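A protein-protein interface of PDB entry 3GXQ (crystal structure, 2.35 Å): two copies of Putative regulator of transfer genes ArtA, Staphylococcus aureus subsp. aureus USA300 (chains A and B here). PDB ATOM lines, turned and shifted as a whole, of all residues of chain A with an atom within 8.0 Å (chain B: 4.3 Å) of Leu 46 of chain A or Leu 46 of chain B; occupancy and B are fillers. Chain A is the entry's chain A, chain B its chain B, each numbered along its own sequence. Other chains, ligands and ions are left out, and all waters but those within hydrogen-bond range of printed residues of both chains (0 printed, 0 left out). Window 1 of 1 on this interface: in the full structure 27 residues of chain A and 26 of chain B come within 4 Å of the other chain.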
ATOM      1  N   LEU A  14     -18.565 -16.617   3.361  1.00  0.00           N
ATOM      2  CA  LEU A  14     -17.426 -16.116   4.116  1.00  0.00           C
ATOM      3  C   LEU A  14     -17.453 -14.664   3.678  1.00  0.00           C
ATOM      4  O   LEU A  14     -17.362 -14.354   2.491  1.00  0.00           O
ATOM      5  CB  LEU A  14     -16.090 -16.767   3.720  1.00  0.00           C
ATOM      6  CG  LEU A  14     -14.893 -16.258   4.557  1.00  0.00           C
ATOM      7  CD1 LEU A  14     -15.014 -16.815   5.962  1.00  0.00           C
ATOM      8  CD2 LEU A  14     -13.544 -16.689   3.963  1.00  0.00           C
ATOM      9  N   LEU A  16     -15.804 -10.904   4.807  1.00  0.00           N
ATOM     10  CA  LEU A  16     -14.943 -10.116   5.666  1.00  0.00           C
ATOM     11  C   LEU A  16     -14.314  -8.900   5.003  1.00  0.00           C
ATOM     12  O   LEU A  16     -14.227  -8.796   3.779  1.00  0.00           O
ATOM     13  CB  LEU A  16     -13.874 -11.005   6.318  1.00  0.00           C
ATOM     14  CG  LEU A  16     -12.680 -11.664   5.620  1.00  0.00           C
ATOM     15  CD1 LEU A  16     -13.047 -12.220   4.248  1.00  0.00           C
ATOM     16  CD2 LEU A  16     -11.598 -10.640   5.540  1.00  0.00           C
ATOM     17  N   LEU A  17     -13.920  -7.953   5.845  1.00  0.00           N
ATOM     18  CA  LEU A  17     -13.303  -6.722   5.388  1.00  0.00           C
ATOM     19  C   LEU A  17     -11.794  -6.948   5.315  1.00  0.00           C
ATOM     20  O   LEU A  17     -11.215  -7.538   6.221  1.00  0.00           O
ATOM     21  CB  LEU A  17     -13.622  -5.590   6.364  1.00  0.00           C
ATOM     22  CG  LEU A  17     -15.106  -5.327   6.636  1.00  0.00           C
ATOM     23  CD1 LEU A  17     -15.244  -4.313   7.771  1.00  0.00           C
ATOM     24  CD2 LEU A  17     -15.795  -4.820   5.370  1.00  0.00           C
ATOM     25  N   VAL A  18     -11.175  -6.494   4.225  1.00  0.00           N
ATOM     26  CA  VAL A  18      -9.727  -6.624   4.019  1.00  0.00           C
ATOM     27  C   VAL A  18      -9.176  -5.300   3.493  1.00  0.00           C
ATOM     28  O   VAL A  18      -9.943  -4.439   3.046  1.00  0.00           O
ATOM     29  CB  VAL A  18      -9.381  -7.736   2.991  1.00  0.00           C
ATOM     30  CG1 VAL A  18      -9.896  -9.070   3.485  1.00  0.00           C
ATOM     31  CG2 VAL A  18      -9.977  -7.412   1.625  1.00  0.00           C
ATOM     32  N   MET A  22      -4.793  -5.793  -0.398  1.00  0.00           N
ATOM     33  CA  MET A  22      -5.021  -7.233  -0.354  1.00  0.00           C
ATOM     34  C   MET A  22      -6.088  -7.682  -1.337  1.00  0.00           C
ATOM     35  O   MET A  22      -5.887  -8.636  -2.079  1.00  0.00           O
ATOM     36  CB  MET A  22      -5.381  -7.696   1.059  1.00  0.00           C
ATOM     37  CG  MET A  22      -5.639  -9.216   1.158  1.00  0.00           C
ATOM     38  SD  MET A  22      -5.644  -9.916   2.837  1.00  0.00           S
ATOM     39  CE  MET A  22      -7.218 -10.439   2.966  1.00  0.00           C
ATOM     40  N   LYS A  23      -7.221  -6.995  -1.360  1.00  0.00           N
ATOM     41  CA  LYS A  23      -8.275  -7.365  -2.285  1.00  0.00           C
ATOM     42  C   LYS A  23      -7.830  -7.213  -3.742  1.00  0.00           C
ATOM     43  O   LYS A  23      -8.283  -7.951  -4.622  1.00  0.00           O
ATOM     44  CB  LYS A  23      -9.524  -6.525  -2.029  1.00  0.00           C
ATOM     45  CG  LYS A  23     -10.680  -6.848  -2.952  1.00  0.00           C
ATOM     46  CD  LYS A  23     -11.969  -6.126  -2.548  1.00  0.00           C
ATOM     47  CE  LYS A  23     -13.156  -6.629  -3.365  1.00  0.00           C
ATOM     48  NZ  LYS A  23     -14.434  -6.044  -2.900  1.00  0.00           N
ATOM     49  N   GLU A  25      -4.716  -7.720  -4.920  1.00  0.00           N
ATOM     50  CA  GLU A  25      -3.819  -8.830  -5.243  1.00  0.00           C
ATOM     51  C   GLU A  25      -4.649 -10.064  -5.577  1.00  0.00           C
ATOM     52  O   GLU A  25      -4.345 -10.813  -6.511  1.00  0.00           O
ATOM     53  CB  GLU A  25      -2.922  -9.157  -4.050  1.00  0.00           C
ATOM     54  CG  GLU A  25      -1.910  -8.087  -3.655  1.00  0.00           C
ATOM     55  CD  GLU A  25      -1.207  -8.442  -2.346  1.00  0.00           C
ATOM     56  OE1 GLU A  25      -1.600  -7.920  -1.284  1.00  0.00           O
ATOM     57  OE2 GLU A  25      -0.266  -9.270  -2.377  1.00  0.00           O
ATOM     58  N   ILE A  26      -5.707 -10.264  -4.799  1.00  0.00           N
ATOM     59  CA  ILE A  26      -6.596 -11.397  -4.981  1.00  0.00           C
ATOM     60  C   ILE A  26      -7.353 -11.311  -6.309  1.00  0.00           C
ATOM     61  O   ILE A  26      -7.611 -12.326  -6.962  1.00  0.00           O
ATOM     62  CB  ILE A  26      -7.588 -11.472  -3.821  1.00  0.00           C
ATOM     63  CG1 ILE A  26      -6.818 -11.652  -2.506  1.00  0.00           C
ATOM     64  CG2 ILE A  26      -8.579 -12.590  -4.060  1.00  0.00           C
ATOM     65  CD1 ILE A  26      -7.730 -11.750  -1.297  1.00  0.00           C
ATOM     66  N   VAL A  38     -13.299 -14.164  -8.581  1.00  0.00           N
ATOM     67  CA  VAL A  38     -12.622 -13.760  -7.347  1.00  0.00           C
ATOM     68  C   VAL A  38     -12.812 -14.733  -6.170  1.00  0.00           C
ATOM     69  O   VAL A  38     -11.887 -15.006  -5.420  1.00  0.00           O
ATOM     70  CB  VAL A  38     -13.069 -12.329  -6.911  1.00  0.00           C
ATOM     71  CG1 VAL A  38     -12.554 -12.004  -5.532  1.00  0.00           C
ATOM     72  CG2 VAL A  38     -12.519 -11.315  -7.902  1.00  0.00           C
ATOM     73  N   SER A  39     -14.009 -15.263  -6.005  1.00  0.00           N
ATOM     74  CA  SER A  39     -14.264 -16.173  -4.899  1.00  0.00           C
ATOM     75  C   SER A  39     -13.449 -17.459  -5.078  1.00  0.00           C
ATOM     76  O   SER A  39     -13.000 -18.062  -4.105  1.00  0.00           O
ATOM     77  CB  SER A  39     -15.761 -16.472  -4.809  1.00  0.00           C
ATOM     78  OG  SER A  39     -16.180 -17.307  -5.867  1.00  0.00           O
ATOM     79  N   GLN A  40     -13.251 -17.867  -6.326  1.00  0.00           N
ATOM     80  CA  GLN A  40     -12.452 -19.053  -6.598  1.00  0.00           C
ATOM     81  C   GLN A  40     -11.019 -18.739  -6.204  1.00  0.00           C
ATOM     82  O   GLN A  40     -10.339 -19.573  -5.612  1.00  0.00           O
ATOM     83  CB  GLN A  40     -12.489 -19.418  -8.077  1.00  0.00           C
ATOM     84  CG  GLN A  40     -11.572 -20.581  -8.446  1.00  0.00           C
ATOM     85  CD  GLN A  40     -11.922 -21.844  -7.690  1.00  0.00           C
ATOM     86  OE1 GLN A  40     -13.097 -22.198  -7.559  1.00  0.00           O
ATOM     87  NE2 GLN A  40     -10.907 -22.541  -7.201  1.00  0.00           N
ATOM     88  N   ALA A  41     -10.569 -17.530  -6.535  1.00  0.00           N
ATOM     89  CA  ALA A  41      -9.208 -17.100  -6.217  1.00  0.00           C
ATOM     90  C   ALA A  41      -9.014 -17.008  -4.708  1.00  0.00           C
ATOM     91  O   ALA A  41      -7.945 -17.306  -4.193  1.00  0.00           O
ATOM     92  CB  ALA A  41      -8.916 -15.744  -6.875  1.00  0.00           C
ATOM     93  N   GLY A  42     -10.062 -16.593  -4.010  1.00  0.00           N
ATOM     94  CA  GLY A  42     -10.000 -16.477  -2.568  1.00  0.00           C
ATOM     95  C   GLY A  42      -9.831 -17.826  -1.891  1.00  0.00           C
ATOM     96  O   GLY A  42      -9.105 -17.940  -0.909  1.00  0.00           O
ATOM     97  N   ARG A  43     -10.481 -18.857  -2.421  1.00  0.00           N
ATOM     98  CA  ARG A  43     -10.375 -20.188  -1.834  1.00  0.00           C
ATOM     99  C   ARG A  43      -8.969 -20.762  -2.013  1.00  0.00           C
ATOM    100  O   ARG A  43      -8.382 -21.281  -1.059  1.00  0.00           O
ATOM    101  CB  ARG A  43     -11.393 -21.143  -2.454  1.00  0.00           C
ATOM    102  CG  ARG A  43     -12.819 -20.652  -2.425  1.00  0.00           C
ATOM    103  CD  ARG A  43     -13.774 -21.765  -2.783  1.00  0.00           C
ATOM    104  NE  ARG A  43     -15.068 -21.224  -3.164  1.00  0.00           N
ATOM    105  CZ  ARG A  43     -15.428 -20.945  -4.411  1.00  0.00           C
ATOM    106  NH1 ARG A  43     -14.592 -21.173  -5.413  1.00  0.00           N
ATOM    107  NH2 ARG A  43     -16.615 -20.406  -4.649  1.00  0.00           N
ATOM    108  N   GLU A  44      -8.434 -20.653  -3.228  1.00  0.00           N
ATOM    109  CA  GLU A  44      -7.091 -21.153  -3.536  1.00  0.00           C
ATOM    110  C   GLU A  44      -6.064 -20.499  -2.620  1.00  0.00           C
ATOM    111  O   GLU A  44      -5.199 -21.175  -2.073  1.00  0.00           O
ATOM    112  CB  GLU A  44      -6.713 -20.849  -4.986  1.00  0.00           C
ATOM    113  CG  GLU A  44      -7.697 -21.350  -6.003  1.00  0.00           C
ATOM    114  CD  GLU A  44      -7.168 -21.286  -7.433  1.00  0.00           C
ATOM    115  OE1 GLU A  44      -6.031 -20.805  -7.657  1.00  0.00           O
ATOM    116  OE2 GLU A  44      -7.903 -21.724  -8.345  1.00  0.00           O
ATOM    117  N   ILE A  45      -6.166 -19.184  -2.456  1.00  0.00           N
ATOM    118  CA  ILE A  45      -5.241 -18.441  -1.613  1.00  0.00           C
ATOM    119  C   ILE A  45      -5.425 -18.837  -0.149  1.00  0.00           C
ATOM    120  O   ILE A  45      -4.448 -19.012   0.578  1.00  0.00           O
ATOM    121  CB  ILE A  45      -5.428 -16.930  -1.830  1.00  0.00           C
ATOM    122  CG1 ILE A  45      -5.060 -16.598  -3.281  1.00  0.00           C
ATOM    123  CG2 ILE A  45      -4.528 -16.125  -0.893  1.00  0.00           C
ATOM    124  CD1 ILE A  45      -5.533 -15.235  -3.761  1.00  0.00           C
ATOM    125  N   LEU A  46      -6.677 -18.993   0.281  1.00  0.00           N
ATOM    126  CA  LEU A  46      -6.966 -19.403   1.655  1.00  0.00           C
ATOM    127  C   LEU A  46      -6.347 -20.800   1.890  1.00  0.00           C
ATOM    128  O   LEU A  46      -5.722 -21.041   2.915  1.00  0.00           O
ATOM    129  CB  LEU A  46      -8.485 -19.432   1.885  1.00  0.00           C
ATOM    130  CG  LEU A  46      -9.207 -18.097   2.153  1.00  0.00           C
ATOM    131  CD1 LEU A  46     -10.700 -18.301   2.092  1.00  0.00           C
ATOM    132  CD2 LEU A  46      -8.829 -17.565   3.520  1.00  0.00           C
ATOM    133  N   LYS A  47      -6.497 -21.702   0.923  1.00  0.00           N
ATOM    134  CA  LYS A  47      -5.936 -23.048   1.027  1.00  0.00           C
ATOM    135  C   LYS A  47      -4.411 -22.973   1.171  1.00  0.00           C
ATOM    136  O   LYS A  47      -3.822 -23.704   1.955  1.00  0.00           O
ATOM    137  CB  LYS A  47      -6.312 -23.858  -0.217  1.00  0.00           C
ATOM    138  CG  LYS A  47      -5.961 -25.342  -0.172  1.00  0.00           C
ATOM    139  CD  LYS A  47      -6.507 -26.061  -1.417  1.00  0.00           C
ATOM    140  CE  LYS A  47      -6.180 -27.562  -1.440  1.00  0.00           C
ATOM    141  NZ  LYS A  47      -6.758 -28.364  -0.316  1.00  0.00           N
ATOM    142  N   LYS A  48      -3.781 -22.075   0.419  1.00  0.00           N
ATOM    143  CA  LYS A  48      -2.332 -21.898   0.478  1.00  0.00           C
ATOM    144  C   LYS A  48      -1.940 -21.322   1.830  1.00  0.00           C
ATOM    145  O   LYS A  48      -0.877 -21.623   2.356  1.00  0.00           O
ATOM    146  CB  LYS A  48      -1.858 -20.946  -0.631  1.00  0.00           C
ATOM    147  CG  LYS A  48      -1.965 -21.488  -2.066  1.00  0.00           C
ATOM    148  CD  LYS A  48      -1.689 -20.377  -3.088  1.00  0.00           C
ATOM    149  CE  LYS A  48      -1.889 -20.827  -4.533  1.00  0.00           C
ATOM    150  NZ  LYS A  48      -0.793 -21.703  -5.048  1.00  0.00           N
ATOM    151  N   GLY A  49      -2.805 -20.482   2.385  1.00  0.00           N
ATOM    152  CA  GLY A  49      -2.522 -19.891   3.676  1.00  0.00           C
ATOM    153  C   GLY A  49      -2.660 -20.935   4.763  1.00  0.00           C
ATOM    154  O   GLY A  49      -1.906 -20.942   5.729  1.00  0.00           O
ATOM    155  N   LEU A  50      -3.624 -21.830   4.592  1.00  0.00           N
ATOM    156  CA  LEU A  50      -3.878 -22.876   5.569  1.00  0.00           C
ATOM    157  C   LEU A  50      -2.764 -23.928   5.693  1.00  0.00           C
ATOM    158  O   LEU A  50      -2.428 -24.352   6.797  1.00  0.00           O
ATOM    159  CB  LEU A  50      -5.223 -23.547   5.273  1.00  0.00           C
ATOM    160  CG  LEU A  50      -6.436 -22.690   5.667  1.00  0.00           C
ATOM    161  CD1 LEU A  50      -7.735 -23.355   5.215  1.00  0.00           C
ATOM    162  CD2 LEU A  50      -6.436 -22.495   7.178  1.00  0.00           C
ATOM    163  N   GLU A  51      -2.171 -24.341   4.581  1.00  0.00           N
ATOM    164  CA  GLU A  51      -1.103 -25.325   4.666  1.00  0.00           C
ATOM    165  C   GLU A  51       0.162 -24.751   5.309  1.00  0.00           C
ATOM    166  O   GLU A  51       1.027 -25.499   5.753  1.00  0.00           O
ATOM    167  CB  GLU A  51      -0.797 -25.916   3.290  1.00  0.00           C
ATOM    168  CG  GLU A  51      -1.309 -25.111   2.136  1.00  0.00           C
ATOM    169  CD  GLU A  51      -1.765 -26.000   1.002  1.00  0.00           C
ATOM    170  OE1 GLU A  51      -2.490 -26.983   1.285  1.00  0.00           O
ATOM    171  OE2 GLU A  51      -1.413 -25.712  -0.162  1.00  0.00           O
ATOM    172  N   GLN A  52       0.256 -23.426   5.373  1.00  0.00           N
ATOM    173  CA  GLN A  52       1.392 -22.761   6.001  1.00  0.00           C
ATOM    174  C   GLN A  52       1.180 -22.744   7.520  1.00  0.00           C
ATOM    175  O   GLN A  52       2.100 -22.469   8.292  1.00  0.00           O
ATOM    176  CB  GLN A  52       1.539 -21.328   5.475  1.00  0.00           C
ATOM    177  CG  GLN A  52       2.001 -20.324   6.530  1.00  0.00           C
ATOM    178  CD  GLN A  52       2.635 -19.066   5.948  1.00  0.00           C
ATOM    179  OE1 GLN A  52       2.537 -18.798   4.748  1.00  0.00           O
ATOM    180  NE2 GLN A  52       3.287 -18.281   6.809  1.00  0.00           N
ATOM    181  N   ILE A  53      -0.043 -23.028   7.951  1.00  0.00           N
ATOM    182  CA  ILE A  53      -0.353 -23.063   9.374  1.00  0.00           C
ATOM    183  C   ILE A  53      -0.005 -24.471   9.818  1.00  0.00           C
ATOM    184  O   ILE A  53       0.649 -24.678  10.840  1.00  0.00           O
ATOM    185  CB  ILE A  53      -1.857 -22.817   9.636  1.00  0.00           C
ATOM    186  CG1 ILE A  53      -2.329 -21.573   8.876  1.00  0.00           C
ATOM    187  CG2 ILE A  53      -2.105 -22.659  11.130  1.00  0.00           C
ATOM    188  CD1 ILE A  53      -1.677 -20.277   9.320  1.00  0.00           C
ATOM    189  N   LEU B  14     -14.941  -8.299   1.112  1.00  0.00           N
ATOM    190  CA  LEU B  14     -14.558  -9.447   0.303  1.00  0.00           C
ATOM    191  C   LEU B  14     -15.627 -10.457   0.675  1.00  0.00           C
ATOM    192  O   LEU B  14     -15.718 -10.860   1.830  1.00  0.00           O
ATOM    193  CB  LEU B  14     -13.182  -9.999   0.703  1.00  0.00           C
ATOM    194  CG  LEU B  14     -12.639 -11.169  -0.135  1.00  0.00           C
ATOM    195  CD1 LEU B  14     -12.316 -10.711  -1.555  1.00  0.00           C
ATOM    196  CD2 LEU B  14     -11.385 -11.709   0.514  1.00  0.00           C
ATOM    197  N   VAL B  18     -17.238 -20.525   0.423  1.00  0.00           N
ATOM    198  CA  VAL B  18     -16.162 -21.458   0.722  1.00  0.00           C
ATOM    199  C   VAL B  18     -16.752 -22.803   1.122  1.00  0.00           C
ATOM    200  O   VAL B  18     -17.893 -22.875   1.595  1.00  0.00           O
ATOM    201  CB  VAL B  18     -15.258 -20.950   1.866  1.00  0.00           C
ATOM    202  CG1 VAL B  18     -14.625 -19.610   1.475  1.00  0.00           C
ATOM    203  CG2 VAL B  18     -16.054 -20.827   3.161  1.00  0.00           C
ATOM    204  N   MET B  22     -13.532 -25.841   4.820  1.00  0.00           N
ATOM    205  CA  MET B  22     -12.531 -24.792   4.902  1.00  0.00           C
ATOM    206  C   MET B  22     -12.937 -23.730   5.906  1.00  0.00           C
ATOM    207  O   MET B  22     -12.095 -23.188   6.618  1.00  0.00           O
ATOM    208  CB  MET B  22     -12.303 -24.155   3.530  1.00  0.00           C
ATOM    209  CG  MET B  22     -11.325 -22.974   3.531  1.00  0.00           C
ATOM    210  SD  MET B  22     -10.765 -22.491   1.868  1.00  0.00           S
ATOM    211  CE  MET B  22     -12.166 -21.742   1.263  1.00  0.00           C
ATOM    212  N   ILE B  26     -11.034 -22.174   9.129  1.00  0.00           N
ATOM    213  CA  ILE B  26     -10.711 -20.767   9.329  1.00  0.00           C
ATOM    214  C   ILE B  26     -11.204 -20.416  10.726  1.00  0.00           C
ATOM    215  O   ILE B  26     -10.561 -19.666  11.450  1.00  0.00           O
ATOM    216  CB  ILE B  26     -11.389 -19.860   8.275  1.00  0.00           C
ATOM    217  CG1 ILE B  26     -10.883 -20.231   6.870  1.00  0.00           C
ATOM    218  CG2 ILE B  26     -11.065 -18.399   8.568  1.00  0.00           C
ATOM    219  CD1 ILE B  26     -11.602 -19.529   5.752  1.00  0.00           C
ATOM    220  N   GLY B  42      -9.216 -14.674   8.644  1.00  0.00           N
ATOM    221  CA  GLY B  42      -9.221 -14.723   7.194  1.00  0.00           C
ATOM    222  C   GLY B  42      -8.169 -13.815   6.564  1.00  0.00           C
ATOM    223  O   GLY B  42      -7.573 -14.168   5.555  1.00  0.00           O
ATOM    224  N   ARG B  43      -7.943 -12.640   7.151  1.00  0.00           N
ATOM    225  CA  ARG B  43      -6.939 -11.699   6.647  1.00  0.00           C
ATOM    226  C   ARG B  43      -5.529 -12.264   6.804  1.00  0.00           C
ATOM    227  O   ARG B  43      -4.737 -12.229   5.861  1.00  0.00           O
ATOM    228  CB  ARG B  43      -7.001 -10.371   7.408  1.00  0.00           C
ATOM    229  CG  ARG B  43      -7.978  -9.354   6.863  1.00  0.00           C
ATOM    230  CD  ARG B  43      -8.125  -8.183   7.827  1.00  0.00           C
ATOM    231  NE  ARG B  43      -9.543  -7.943   8.014  1.00  0.00           N
ATOM    232  CZ  ARG B  43     -10.146  -7.784   9.180  1.00  0.00           C
ATOM    233  NH1 ARG B  43      -9.461  -7.816  10.316  1.00  0.00           N
ATOM    234  NH2 ARG B  43     -11.457  -7.651   9.189  1.00  0.00           N
ATOM    235  N   GLU B  44      -5.221 -12.764   8.003  1.00  0.00           N
ATOM    236  CA  GLU B  44      -3.912 -13.339   8.299  1.00  0.00           C
ATOM    237  C   GLU B  44      -3.645 -14.541   7.393  1.00  0.00           C
ATOM    238  O   GLU B  44      -2.550 -14.709   6.868  1.00  0.00           O
ATOM    239  CB  GLU B  44      -3.837 -13.781   9.766  1.00  0.00           C
ATOM    240  CG  GLU B  44      -4.302 -12.730  10.761  1.00  0.00           C
ATOM    241  CD  GLU B  44      -4.267 -13.217  12.205  1.00  0.00           C
ATOM    242  OE1 GLU B  44      -4.656 -14.382  12.452  1.00  0.00           O
ATOM    243  OE2 GLU B  44      -3.865 -12.431  13.095  1.00  0.00           O
ATOM    244  N   ILE B  45      -4.661 -15.373   7.216  1.00  0.00           N
ATOM    245  CA  ILE B  45      -4.552 -16.554   6.377  1.00  0.00           C
ATOM    246  C   ILE B  45      -4.358 -16.155   4.923  1.00  0.00           C
ATOM    247  O   ILE B  45      -3.478 -16.670   4.237  1.00  0.00           O
ATOM    248  CB  ILE B  45      -5.804 -17.419   6.525  1.00  0.00           C
ATOM    249  CG1 ILE B  45      -5.880 -17.923   7.970  1.00  0.00           C
ATOM    250  CG2 ILE B  45      -5.785 -18.580   5.528  1.00  0.00           C
ATOM    251  CD1 ILE B  45      -7.196 -18.605   8.319  1.00  0.00           C
ATOM    252  N   LEU B  46      -5.179 -15.228   4.453  1.00  0.00           N
ATOM    253  CA  LEU B  46      -5.063 -14.770   3.083  1.00  0.00           C
ATOM    254  C   LEU B  46      -3.675 -14.179   2.833  1.00  0.00           C
ATOM    255  O   LEU B  46      -3.080 -14.388   1.779  1.00  0.00           O
ATOM    256  CB  LEU B  46      -6.145 -13.727   2.776  1.00  0.00           C
ATOM    257  CG  LEU B  46      -7.543 -14.269   2.457  1.00  0.00           C
ATOM    258  CD1 LEU B  46      -8.554 -13.136   2.425  1.00  0.00           C
ATOM    259  CD2 LEU B  46      -7.520 -14.986   1.116  1.00  0.00           C
ATOM    260  N   LYS B  47      -3.158 -13.448   3.812  1.00  0.00           N
ATOM    261  CA  LYS B  47      -1.854 -12.824   3.669  1.00  0.00           C
ATOM    262  C   LYS B  47      -0.740 -13.860   3.535  1.00  0.00           C
ATOM    263  O   LYS B  47       0.191 -13.681   2.752  1.00  0.00           O
ATOM    264  CB  LYS B  47      -1.575 -11.897   4.858  1.00  0.00           C
ATOM    265  CG  LYS B  47      -0.221 -11.219   4.783  1.00  0.00           C
ATOM    266  CD  LYS B  47      -0.053 -10.507   3.442  1.00  0.00           C
ATOM    267  CE  LYS B  47       1.362  -9.992   3.247  1.00  0.00           C
ATOM    268  NZ  LYS B  47       1.485  -9.243   1.961  1.00  0.00           N
ATOM    269  N   LYS B  48      -0.827 -14.943   4.299  1.00  0.00           N
ATOM    270  CA  LYS B  48       0.181 -15.979   4.210  1.00  0.00           C
ATOM    271  C   LYS B  48       0.088 -16.612   2.832  1.00  0.00           C
ATOM    272  O   LYS B  48       1.106 -16.917   2.208  1.00  0.00           O
ATOM    273  CB  LYS B  48      -0.042 -17.036   5.287  1.00  0.00           C
ATOM    274  CG  LYS B  48       0.125 -16.515   6.700  1.00  0.00           C
ATOM    275  CD  LYS B  48      -0.323 -17.556   7.727  1.00  0.00           C
ATOM    276  CE  LYS B  48      -0.174 -17.054   9.159  1.00  0.00           C
ATOM    277  NZ  LYS B  48       1.245 -16.768   9.519  1.00  0.00           N
ATOM    278  N   GLY B  49      -1.138 -16.802   2.355  1.00  0.00           N
ATOM    279  CA  GLY B  49      -1.330 -17.402   1.048  1.00  0.00           C
ATOM    280  C   GLY B  49      -0.775 -16.527  -0.055  1.00  0.00           C
ATOM    281  O   GLY B  49      -0.186 -17.019  -1.021  1.00  0.00           O
ATOM    282  N   LEU B  50      -0.973 -15.220   0.089  1.00  0.00           N
ATOM    283  CA  LEU B  50      -0.491 -14.256  -0.891  1.00  0.00           C
ATOM    284  C   LEU B  50       1.031 -14.194  -0.883  1.00  0.00           C
ATOM    285  O   LEU B  50       1.654 -13.988  -1.921  1.00  0.00           O
ATOM    286  CB  LEU B  50      -1.081 -12.870  -0.604  1.00  0.00           C
ATOM    287  CG  LEU B  50      -2.556 -12.728  -0.993  1.00  0.00           C
ATOM    288  CD1 LEU B  50      -3.128 -11.464  -0.405  1.00  0.00           C
ATOM    289  CD2 LEU B  50      -2.686 -12.724  -2.508  1.00  0.00           C
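Leu 14 of chain A touches Ile 26 of chain B, but with the chains exchanged Ile 26 of chain A does not touch Leu 14 of chain B (4.1 Å). Ile 45 of chain A touches Gly 49 of chain B, and with the chains exchanged Gly 49 of chain A touches Ile 45 of chain B. Ile 45 of chain A touches Leu 50 of chain B, but with the chains exchanged Leu 50 of chain A does not touch Ile 45 of chain B (4.01 Å). Lys 48 of chain A touches Gly 49 of chain B, but with the chains exchanged Gly 49 of chain A does not touch Lys 48 of chain B (4.1 Å). 13 positions are printed for both chains.
The side-chain hydroxyl of Ser 39 of chain A lies within hydrogen-bond range of the guanidinium group of Arg 43 of chain A, 3.4 Å away. The side-chain amide oxygen (OE1) of Gln 40 of chain A lies within hydrogen-bond range of the guanidinium group (NH1) of Arg 43 of chain A (2.8 Å).
Of chain B, only Met 22 (3.8 Å), Ile 26 (3.96 Å), Ile 45 (3.6 Å) and Leu 46 (3.7 Å) come within 4 Å of Leu 46 of chain A. Printed residues of chain B within 4 Å of Gly 42 of chain A: Leu 46 (3.9 Å). Of the printed residues of chain A, Lys 48 of chain B touches Gln 52 (3.2 Å) and Ile 53 (3.4 Å). Of the printed residues of chain A, Gly 49 of chain B touches Ile 45 (3.5 Å), Lys 48 (3.96 Å) and Gly 49 (3.6 Å). Of the printed residues of chain B, Ile 53 of chain A touches Lys 48 (3.4 Å). Lys 47 of chain A touches none of the printed residues of chain B. The nearest printed residue of chain B that does not touch Leu 46 of chain A is Gly 42 of chain B (4.2 Å). The nearest residue of chain A that does not touch Leu 46 of chain B is Ile 26 of chain A (4.04 Å).
Among the printed residues, pairs that only touch across the chains: Leu 14 of chain A with Leu 14 of chain B (3.9 Å), Leu 14 of chain A with Val 18 of chain B (3.9 Å), Leu 14 of chain A with Ile 26 of chain B (3.9 Å), Val 18 of chain A with Arg 43 of chain B (3.9 Å), Met 22 of chain A with Arg 43 of chain B (3.9 Å), Met 22 of chain A with Leu 46 of chain B (3.1 Å), Met 22 of chain A with Leu 50 of chain B (3.7 Å), Glu 25 of chain A with Leu 50 of chain B (3.9 Å), Gly 42 of chain A with Leu 46 of chain B (3.9 Å), Arg 43 of chain A with Met 22 of chain B (3.8 Å), Ile 45 of chain A with Leu 46 of chain B (3.5 Å), Ile 45 of chain A with Gly 49 of chain B (3.5 Å), Ile 45 of chain A with Leu 50 of chain B (3.8 Å), Leu 46 of chain A with Met 22 of chain B (3.8 Å), Leu 46 of chain A with Ile 26 of chain B (3.96 Å), Leu 46 of chain A with Ile 45 of chain B (3.6 Å), Leu 46 of chain A with Leu 46 of chain B (3.7 Å), Lys 48 of chain A with Gly 49 of chain B (3.96 Å), Gly 49 of chain A with Ile 45 of chain B (3.4 Å), Gly 49 of chain A with Gly 49 of chain B (3.6 Å), Leu 50 of chain A with Met 22 of chain B (3.98 Å) and Ile 53 of chain A with Lys 48 of chain B (3.4 Å).
The backbone carbonyl oxygen (O) of Leu 16 of chain A sits at hydrogen-bond distance from the backbone NH (N) of Leu 14 of chain B. NE of Arg 43 of chain B is in hydrogen-bond range of O of Leu 17 of chain A, at 2.5 Å. O of Lys 48 of chain B lies close to OE1 of Gln 52 of chain A.
Printed residues of chain B that touch a printed residue of chain A: Leu 14, Val 18, Met 22, Ile 26, Arg 43, Ile 45, Leu 46, Lys 48, Gly 49 and Leu 50. Of the 24 printed residues of chain A, 15 touch a printed residue of chain B. Along chain A the printed residues that touch a printed residue of chain B span positions 14 to 53.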
